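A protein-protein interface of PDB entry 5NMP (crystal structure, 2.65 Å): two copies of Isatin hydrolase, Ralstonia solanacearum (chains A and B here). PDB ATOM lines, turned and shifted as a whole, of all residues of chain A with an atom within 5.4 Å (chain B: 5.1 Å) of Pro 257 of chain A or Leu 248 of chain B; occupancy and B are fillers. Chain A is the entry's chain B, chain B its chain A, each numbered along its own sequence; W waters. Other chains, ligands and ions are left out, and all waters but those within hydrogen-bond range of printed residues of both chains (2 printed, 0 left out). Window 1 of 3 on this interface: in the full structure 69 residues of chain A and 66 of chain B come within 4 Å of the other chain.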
ATOM      1  N   LEU A  32       2.324  12.519  -5.273  1.00  0.00           N
ATOM      2  CA  LEU A  32       2.239  12.090  -6.667  1.00  0.00           C
ATOM      3  C   LEU A  32       0.794  12.085  -7.149  1.00  0.00           C
ATOM      4  O   LEU A  32      -0.035  11.327  -6.648  1.00  0.00           O
ATOM      5  CB  LEU A  32       2.855  10.702  -6.845  1.00  0.00           C
ATOM      6  CG  LEU A  32       4.381  10.600  -6.819  1.00  0.00           C
ATOM      7  CD1 LEU A  32       4.808   9.171  -6.531  1.00  0.00           C
ATOM      8  CD2 LEU A  32       4.969  11.076  -8.139  1.00  0.00           C
ATOM      9  N   PHE A  71      -0.258   2.314 -12.038  1.00  0.00           N
ATOM     10  CA  PHE A  71       0.217   3.657 -12.362  1.00  0.00           C
ATOM     11  C   PHE A  71       1.410   3.643 -13.313  1.00  0.00           C
ATOM     12  O   PHE A  71       2.089   2.627 -13.475  1.00  0.00           O
ATOM     13  CB  PHE A  71       0.577   4.425 -11.086  1.00  0.00           C
ATOM     14  CG  PHE A  71       1.823   3.931 -10.403  1.00  0.00           C
ATOM     15  CD1 PHE A  71       3.034   4.582 -10.578  1.00  0.00           C
ATOM     16  CD2 PHE A  71       1.781   2.821  -9.573  1.00  0.00           C
ATOM     17  CE1 PHE A  71       4.180   4.130  -9.947  1.00  0.00           C
ATOM     18  CE2 PHE A  71       2.923   2.367  -8.939  1.00  0.00           C
ATOM     19  CZ  PHE A  71       4.124   3.022  -9.126  1.00  0.00           C
ATOM     20  N   CYS A  73       4.665   6.454 -14.820  1.00  0.00           N
ATOM     21  CA  CYS A  73       5.336   7.742 -14.776  1.00  0.00           C
ATOM     22  C   CYS A  73       6.743   7.594 -15.332  1.00  0.00           C
ATOM     23  O   CYS A  73       7.012   6.710 -16.145  1.00  0.00           O
ATOM     24  CB  CYS A  73       5.374   8.291 -13.348  1.00  0.00           C
ATOM     25  SG  CYS A  73       6.159   7.200 -12.131  1.00  0.00           S
ATOM     26  N   GLY A  74       7.640   8.464 -14.891  1.00  0.00           N
ATOM     27  CA  GLY A  74       9.028   8.373 -15.284  1.00  0.00           C
ATOM     28  C   GLY A  74       9.898   8.242 -14.055  1.00  0.00           C
ATOM     29  O   GLY A  74       9.432   8.433 -12.931  1.00  0.00           O
ATOM     30  N   GLU A  75      11.163   7.902 -14.264  1.00  0.00           N
ATOM     31  CA  GLU A  75      12.126   7.887 -13.176  1.00  0.00           C
ATOM     32  C   GLU A  75      12.269   9.288 -12.581  1.00  0.00           C
ATOM     33  O   GLU A  75      12.502   9.449 -11.384  1.00  0.00           O
ATOM     34  CB  GLU A  75      13.477   7.374 -13.670  1.00  0.00           C
ATOM     35  CG  GLU A  75      13.440   5.970 -14.247  1.00  0.00           C
ATOM     36  CD  GLU A  75      14.771   5.559 -14.854  1.00  0.00           C
ATOM     37  OE1 GLU A  75      15.458   6.423 -15.440  1.00  0.00           O
ATOM     38  OE2 GLU A  75      15.134   4.371 -14.739  1.00  0.00           O
ATOM     39  N   HIS A  76      12.115  10.306 -13.420  1.00  0.00           N
ATOM     40  CA  HIS A  76      12.274  11.681 -12.970  1.00  0.00           C
ATOM     41  C   HIS A  76      10.931  12.401 -12.856  1.00  0.00           C
ATOM     42  O   HIS A  76      10.694  13.412 -13.512  1.00  0.00           O
ATOM     43  CB  HIS A  76      13.220  12.428 -13.911  1.00  0.00           C
ATOM     44  CG  HIS A  76      14.590  11.828 -13.975  1.00  0.00           C
ATOM     45  ND1 HIS A  76      15.678  12.385 -13.338  1.00  0.00           N
ATOM     46  CD2 HIS A  76      15.042  10.701 -14.575  1.00  0.00           C
ATOM     47  CE1 HIS A  76      16.743  11.634 -13.553  1.00  0.00           C
ATOM     48  NE2 HIS A  76      16.385  10.605 -14.301  1.00  0.00           N
ATOM     49  N   THR A  77      10.064  11.867 -12.000  1.00  0.00           N
ATOM     50  CA  THR A  77       8.737  12.427 -11.772  1.00  0.00           C
ATOM     51  C   THR A  77       8.582  12.877 -10.321  1.00  0.00           C
ATOM     52  O   THR A  77       8.917  12.134  -9.396  1.00  0.00           O
ATOM     53  CB  THR A  77       7.626  11.405 -12.112  1.00  0.00           C
ATOM     54  OG1 THR A  77       7.633  11.134 -13.520  1.00  0.00           O
ATOM     55  CG2 THR A  77       6.257  11.940 -11.716  1.00  0.00           C
ATOM     56  N   THR A  79       8.959  14.410  -6.671  1.00  0.00           N
ATOM     57  CA  THR A  79      10.108  14.289  -5.787  1.00  0.00           C
ATOM     58  C   THR A  79      10.902  13.048  -6.172  1.00  0.00           C
ATOM     59  O   THR A  79      10.490  11.926  -5.875  1.00  0.00           O
ATOM     60  CB  THR A  79       9.686  14.195  -4.314  1.00  0.00           C
ATOM     61  OG1 THR A  79       8.736  15.224  -4.019  1.00  0.00           O
ATOM     62  CG2 THR A  79      10.892  14.348  -3.403  1.00  0.00           C
ATOM     63  N   HIS A  80      12.033  13.243  -6.844  1.00  0.00           N
ATOM     64  CA  HIS A  80      12.795  12.101  -7.326  1.00  0.00           C
ATOM     65  C   HIS A  80      14.290  12.212  -7.058  1.00  0.00           C
ATOM     66  O   HIS A  80      14.784  13.231  -6.573  1.00  0.00           O
ATOM     67  CB  HIS A  80      12.545  11.889  -8.825  1.00  0.00           C
ATOM     68  CG  HIS A  80      13.189  12.912  -9.708  1.00  0.00           C
ATOM     69  ND1 HIS A  80      12.526  14.039 -10.147  1.00  0.00           N
ATOM     70  CD2 HIS A  80      14.425  12.965 -10.257  1.00  0.00           C
ATOM     71  CE1 HIS A  80      13.333  14.748 -10.917  1.00  0.00           C
ATOM     72  NE2 HIS A  80      14.491  14.118 -11.000  1.00  0.00           N
ATOM     73  N   PHE A  81      14.994  11.135  -7.390  1.00  0.00           N
ATOM     74  CA  PHE A  81      16.405  10.961  -7.081  1.00  0.00           C
ATOM     75  C   PHE A  81      17.200  10.876  -8.377  1.00  0.00           C
ATOM     76  O   PHE A  81      16.848  10.105  -9.267  1.00  0.00           O
ATOM     77  CB  PHE A  81      16.584   9.698  -6.230  1.00  0.00           C
ATOM     78  CG  PHE A  81      18.011   9.366  -5.891  1.00  0.00           C
ATOM     79  CD1 PHE A  81      18.580   9.816  -4.712  1.00  0.00           C
ATOM     80  CD2 PHE A  81      18.767   8.562  -6.727  1.00  0.00           C
ATOM     81  CE1 PHE A  81      19.888   9.496  -4.388  1.00  0.00           C
ATOM     82  CE2 PHE A  81      20.074   8.240  -6.409  1.00  0.00           C
ATOM     83  CZ  PHE A  81      20.634   8.707  -5.236  1.00  0.00           C
ATOM     84  N   ALA A 246      16.018   6.705  -0.067  1.00  0.00           N
ATOM     85  CA  ALA A 246      16.315   5.473  -0.781  1.00  0.00           C
ATOM     86  C   ALA A 246      15.452   5.356  -2.033  1.00  0.00           C
ATOM     87  O   ALA A 246      14.226   5.331  -1.947  1.00  0.00           O
ATOM     88  CB  ALA A 246      16.111   4.275   0.126  1.00  0.00           C
ATOM     89  N   PRO A 247      16.098   5.300  -3.207  1.00  0.00           N
ATOM     90  CA  PRO A 247      15.393   5.179  -4.487  1.00  0.00           C
ATOM     91  C   PRO A 247      14.935   3.755  -4.779  1.00  0.00           C
ATOM     92  O   PRO A 247      15.504   2.801  -4.244  1.00  0.00           O
ATOM     93  CB  PRO A 247      16.443   5.630  -5.504  1.00  0.00           C
ATOM     94  CG  PRO A 247      17.740   5.303  -4.867  1.00  0.00           C
ATOM     95  CD  PRO A 247      17.546   5.502  -3.390  1.00  0.00           C
ATOM     96  N   LEU A 248      13.907   3.625  -5.614  1.00  0.00           N
ATOM     97  CA  LEU A 248      13.423   2.323  -6.052  1.00  0.00           C
ATOM     98  C   LEU A 248      14.535   1.544  -6.737  1.00  0.00           C
ATOM     99  O   LEU A 248      15.369   2.122  -7.432  1.00  0.00           O
ATOM    100  CB  LEU A 248      12.238   2.481  -7.005  1.00  0.00           C
ATOM    101  CG  LEU A 248      10.996   3.183  -6.465  1.00  0.00           C
ATOM    102  CD1 LEU A 248       9.931   3.276  -7.548  1.00  0.00           C
ATOM    103  CD2 LEU A 248      10.469   2.449  -5.249  1.00  0.00           C
ATOM    104  N   GLY A 255      17.384   6.838 -12.104  1.00  0.00           N
ATOM    105  CA  GLY A 255      16.788   7.569 -11.005  1.00  0.00           C
ATOM    106  C   GLY A 255      15.426   6.992 -10.692  1.00  0.00           C
ATOM    107  O   GLY A 255      15.014   6.010 -11.308  1.00  0.00           O
ATOM    108  N   SER A 256      14.729   7.596  -9.737  1.00  0.00           N
ATOM    109  CA  SER A 256      13.370   7.181  -9.404  1.00  0.00           C
ATOM    110  C   SER A 256      12.702   8.193  -8.486  1.00  0.00           C
ATOM    111  O   SER A 256      13.381   8.941  -7.784  1.00  0.00           O
ATOM    112  CB  SER A 256      13.365   5.803  -8.734  1.00  0.00           C
ATOM    113  OG  SER A 256      13.650   5.909  -7.351  1.00  0.00           O
ATOM    114  N   PRO A 257      11.362   8.222  -8.494  1.00  0.00           N
ATOM    115  CA  PRO A 257      10.649   8.898  -7.410  1.00  0.00           C
ATOM    116  C   PRO A 257      10.934   8.190  -6.091  1.00  0.00           C
ATOM    117  O   PRO A 257      11.248   6.997  -6.099  1.00  0.00           O
ATOM    118  CB  PRO A 257       9.178   8.756  -7.809  1.00  0.00           C
ATOM    119  CG  PRO A 257       9.148   7.568  -8.720  1.00  0.00           C
ATOM    120  CD  PRO A 257      10.439   7.639  -9.481  1.00  0.00           C
ATOM    121  N   LEU A 258      10.832   8.908  -4.977  1.00  0.00           N
ATOM    122  CA  LEU A 258      11.081   8.296  -3.679  1.00  0.00           C
ATOM    123  C   LEU A 258      10.450   9.098  -2.551  1.00  0.00           C
ATOM    124  O   LEU A 258      10.103  10.263  -2.723  1.00  0.00           O
ATOM    125  CB  LEU A 258      12.586   8.139  -3.432  1.00  0.00           C
ATOM    126  CG  LEU A 258      13.425   9.345  -3.002  1.00  0.00           C
ATOM    127  CD1 LEU A 258      14.854   8.899  -2.736  1.00  0.00           C
ATOM    128  CD2 LEU A 258      13.408  10.471  -4.033  1.00  0.00           C
ATOM    129  N   ARG A 259      10.293   8.455  -1.399  1.00  0.00           N
ATOM    130  CA  ARG A 259       9.806   9.128  -0.204  1.00  0.00           C
ATOM    131  C   ARG A 259      10.996   9.671   0.566  1.00  0.00           C
ATOM    132  O   ARG A 259      11.730   8.909   1.197  1.00  0.00           O
ATOM    133  CB  ARG A 259       8.991   8.170   0.671  1.00  0.00           C
ATOM    134  CG  ARG A 259       8.089   8.851   1.706  1.00  0.00           C
ATOM    135  CD  ARG A 259       7.007   9.670   1.022  1.00  0.00           C
ATOM    136  NE  ARG A 259       6.046  10.256   1.954  1.00  0.00           N
ATOM    137  CZ  ARG A 259       4.859   9.728   2.241  1.00  0.00           C
ATOM    138  NH1 ARG A 259       4.476   8.589   1.677  1.00  0.00           N
ATOM    139  NH2 ARG A 259       4.052  10.340   3.096  1.00  0.00           N
ATOM    140  N   PHE B  71       8.446   4.192 -16.793  1.00  0.00           N
ATOM    141  CA  PHE B  71       8.023   2.867 -16.346  1.00  0.00           C
ATOM    142  C   PHE B  71       6.560   2.821 -15.923  1.00  0.00           C
ATOM    143  O   PHE B  71       5.934   3.849 -15.660  1.00  0.00           O
ATOM    144  CB  PHE B  71       8.913   2.366 -15.197  1.00  0.00           C
ATOM    145  CG  PHE B  71       8.736   3.115 -13.902  1.00  0.00           C
ATOM    146  CD1 PHE B  71       7.922   2.607 -12.898  1.00  0.00           C
ATOM    147  CD2 PHE B  71       9.404   4.309 -13.674  1.00  0.00           C
ATOM    148  CE1 PHE B  71       7.765   3.284 -11.700  1.00  0.00           C
ATOM    149  CE2 PHE B  71       9.253   4.991 -12.477  1.00  0.00           C
ATOM    150  CZ  PHE B  71       8.431   4.478 -11.490  1.00  0.00           C
ATOM    151  N   VAL B  98      -1.005   5.653   1.589  1.00  0.00           N
ATOM    152  CA  VAL B  98       0.437   5.905   1.645  1.00  0.00           C
ATOM    153  C   VAL B  98       0.795   7.392   1.625  1.00  0.00           C
ATOM    154  O   VAL B  98       1.920   7.770   1.950  1.00  0.00           O
ATOM    155  CB  VAL B  98       1.182   5.200   0.486  1.00  0.00           C
ATOM    156  CG1 VAL B  98       1.237   3.698   0.720  1.00  0.00           C
ATOM    157  CG2 VAL B  98       0.535   5.521  -0.852  1.00  0.00           C
ATOM    158  N   ASP B  99      -0.161   8.235   1.252  1.00  0.00           N
ATOM    159  CA  ASP B  99       0.064   9.673   1.247  1.00  0.00           C
ATOM    160  C   ASP B  99      -0.432  10.344   2.531  1.00  0.00           C
ATOM    161  O   ASP B  99      -0.138  11.514   2.773  1.00  0.00           O
ATOM    162  CB  ASP B  99      -0.612  10.314   0.031  1.00  0.00           C
ATOM    163  CG  ASP B  99      -2.115  10.091   0.014  1.00  0.00           C
ATOM    164  OD1 ASP B  99      -2.557   9.010   0.453  1.00  0.00           O
ATOM    165  OD2 ASP B  99      -2.854  10.994  -0.438  1.00  0.00           O
ATOM    166  N   ALA B 246       9.711   3.552   3.713  1.00  0.00           N
ATOM    167  CA  ALA B 246       8.865   4.677   3.337  1.00  0.00           C
ATOM    168  C   ALA B 246       8.328   4.512   1.915  1.00  0.00           C
ATOM    169  O   ALA B 246       9.099   4.454   0.954  1.00  0.00           O
ATOM    170  CB  ALA B 246       9.632   5.981   3.468  1.00  0.00           C
ATOM    171  N   PRO B 247       6.996   4.435   1.781  1.00  0.00           N
ATOM    172  CA  PRO B 247       6.329   4.248   0.489  1.00  0.00           C
ATOM    173  C   PRO B 247       6.190   5.552  -0.292  1.00  0.00           C
ATOM    174  O   PRO B 247       6.219   6.628   0.305  1.00  0.00           O
ATOM    175  CB  PRO B 247       4.957   3.709   0.888  1.00  0.00           C
ATOM    176  CG  PRO B 247       4.691   4.356   2.214  1.00  0.00           C
ATOM    177  CD  PRO B 247       6.034   4.481   2.897  1.00  0.00           C
ATOM    178  N   LEU B 248       6.041   5.450  -1.611  1.00  0.00           N
ATOM    179  CA  LEU B 248       5.827   6.625  -2.449  1.00  0.00           C
ATOM    180  C   LEU B 248       4.572   7.375  -2.013  1.00  0.00           C
ATOM    181  O   LEU B 248       3.584   6.763  -1.607  1.00  0.00           O
ATOM    182  CB  LEU B 248       5.708   6.227  -3.919  1.00  0.00           C
ATOM    183  CG  LEU B 248       6.844   5.406  -4.519  1.00  0.00           C
ATOM    184  CD1 LEU B 248       6.511   5.037  -5.951  1.00  0.00           C
ATOM    185  CD2 LEU B 248       8.152   6.177  -4.452  1.00  0.00           C
ATOM    186  N   LYS B 249       4.610   8.699  -2.103  1.00  0.00           N
ATOM    187  CA  LYS B 249       3.470   9.512  -1.701  1.00  0.00           C
ATOM    188  C   LYS B 249       2.415   9.563  -2.807  1.00  0.00           C
ATOM    189  O   LYS B 249       2.105  10.630  -3.338  1.00  0.00           O
ATOM    190  CB  LYS B 249       3.924  10.922  -1.325  1.00  0.00           C
ATOM    191  CG  LYS B 249       2.949  11.654  -0.423  1.00  0.00           C
ATOM    192  CD  LYS B 249       3.558  12.920   0.143  1.00  0.00           C
ATOM    193  CE  LYS B 249       2.617  13.571   1.143  1.00  0.00           C
ATOM    194  NZ  LYS B 249       3.133  14.881   1.627  1.00  0.00           N
ATOM    195  N   ILE B 250       1.874   8.394  -3.142  1.00  0.00           N
ATOM    196  CA  ILE B 250       0.842   8.265  -4.167  1.00  0.00           C
ATOM    197  C   ILE B 250      -0.514   8.713  -3.632  1.00  0.00           C
ATOM    198  O   ILE B 250      -0.994   8.184  -2.627  1.00  0.00           O
ATOM    199  CB  ILE B 250       0.732   6.808  -4.672  1.00  0.00           C
ATOM    200  CG1 ILE B 250       2.093   6.310  -5.165  1.00  0.00           C
ATOM    201  CG2 ILE B 250      -0.327   6.688  -5.761  1.00  0.00           C
ATOM    202  CD1 ILE B 250       2.058   4.916  -5.739  1.00  0.00           C
ATOM    203  N   SER B 256       2.538   0.886  -2.249  1.00  0.00           N
ATOM    204  CA  SER B 256       3.491   1.213  -3.306  1.00  0.00           C
ATOM    205  C   SER B 256       4.738   0.357  -3.197  1.00  0.00           C
ATOM    206  O   SER B 256       5.074  -0.120  -2.113  1.00  0.00           O
ATOM    207  CB  SER B 256       3.881   2.698  -3.264  1.00  0.00           C
ATOM    208  OG  SER B 256       4.944   2.932  -2.356  1.00  0.00           O
ATOM    209  N   PRO B 257       5.423   0.145  -4.326  1.00  0.00           N
ATOM    210  CA  PRO B 257       6.767  -0.426  -4.229  1.00  0.00           C
ATOM    211  C   PRO B 257       7.668   0.548  -3.484  1.00  0.00           C
ATOM    212  O   PRO B 257       7.414   1.752  -3.514  1.00  0.00           O
ATOM    213  CB  PRO B 257       7.192  -0.598  -5.689  1.00  0.00           C
ATOM    214  CG  PRO B 257       6.293   0.301  -6.465  1.00  0.00           C
ATOM    215  CD  PRO B 257       5.001   0.349  -5.721  1.00  0.00           C
HETATM  216  O   HOH W   1       7.106   9.845  -3.511  1.00  0.00           O
HETATM  217  O   HOH W   2       2.008   9.416   4.395  1.00  0.00           O
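Of the 18 printed residues of chain A, 8 touch a printed residue of chain B. Hydrophobic or aromatic side chains of chain A within 4 Å of the printed part of chain B: Leu 32 and Leu 248. Of the 10 printed residues of chain B, 7 touch a printed residue of chain A. Hydrophobic or aromatic side chains of chain B within 4 Å of the printed part of chain A: Phe 71, Ala 246 and Leu 248. Among the printed residues, 12 pairs touch across the chains.
The backbone carbonyl oxygen of Lys 249 of chain B sits at hydrogen-bond distance from the backbone NH of Leu 32 of chain A (2.7 Å). The backbone NH (N) of Phe 71 of chain B sits at hydrogen-bond distance from the backbone carbonyl oxygen (O) of Cys 73 of chain A (3.0 Å). The backbone carbonyl oxygen (O) of Val 98 of chain B is in hydrogen-bond range of the guanidinium group (NH1) of Arg 259 of chain A, at 2.7 Å. NH1 of Arg 259 of chain A lies within hydrogen-bond range of O of Pro 247 of chain B.
Phe 71 of chain B touches Gly 74 of chain A (CE2 to O, 3.5 Å). Glu 75 of chain A touches Phe 71 of chain B. Leu 248 of chain A touches Pro 257 of chain B. O of Pro 257 of chain A touches CD2 of Leu 248 of chain B (3.6 Å). Leu 258 of chain A touches Leu 248 of chain B (CA to CD2, 3.7 Å). CB of Arg 259 of chain A touches CB of Ala 246 of chain B, 3.6 Å away. NH1 of Arg 259 of chain A touches O of Leu 248 of chain B, 3.9 Å away. Lys 249 of chain B touches Arg 259 of chain A.
O of Thr 79 of chain A is in hydrogen-bond range of N of Leu 258 of chain A (3.2 Å). N of Leu 248 of chain A lies within hydrogen-bond range of OG of Ser 256 of chain A, 2.9 Å away. The backbone NH (N) of Leu 248 of chain B is in hydrogen-bond range of the side-chain hydroxyl (OG) of Ser 256 of chain B (2.8 Å). The backbone NH of Ser 256 of chain A sits close to the backbone carbonyl oxygen of Glu 75 of chain A (3.3 Å). The side-chain hydroxyl (OG1) of Thr 77 of chain A sits at hydrogen-bond distance from the backbone NH (N) of Gly 74 of chain A, 3.0 Å away.
Of the printed residues of chain B, Leu 248 of chain A touches Pro 257. Pro 257 of chain A touches just one residue of chain B: Leu 248 (3.6 Å). Of the printed residues of chain A, Ala 246 of chain B touches Arg 259. Of chain A, only Pro 257, Leu 258 and Arg 259 come within 4 Å of Leu 248 of chain B. Ser 256 of chain B touches none of the printed residues of chain A. The nearest residue of chain A that does not touch Leu 248 of chain B is Leu 32 of chain A (4.04 Å). The nearest printed residue of chain B that does not touch Gly 74 of chain A is Leu 248 of chain B (8.3 Å).
Leu 248 of chain A touches Pro 257 of chain B, and with the chains exchanged Pro 257 of chain A touches Leu 248 of chain B. Positions printed for both chains: 71, 246, 247, 248, 256 and 257.
Water W2 lies within hydrogen-bond range of NH2 of Arg 259 of chain A (2.6 Å), O of Val 98 of chain B (2.9 Å) and O of Asp 99 of chain B (3.4 Å). Water W1 lies within hydrogen-bond range of N of Lys 249 of chain B (3.1 Å) and O of Leu 258 of chain A (3.1 Å).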
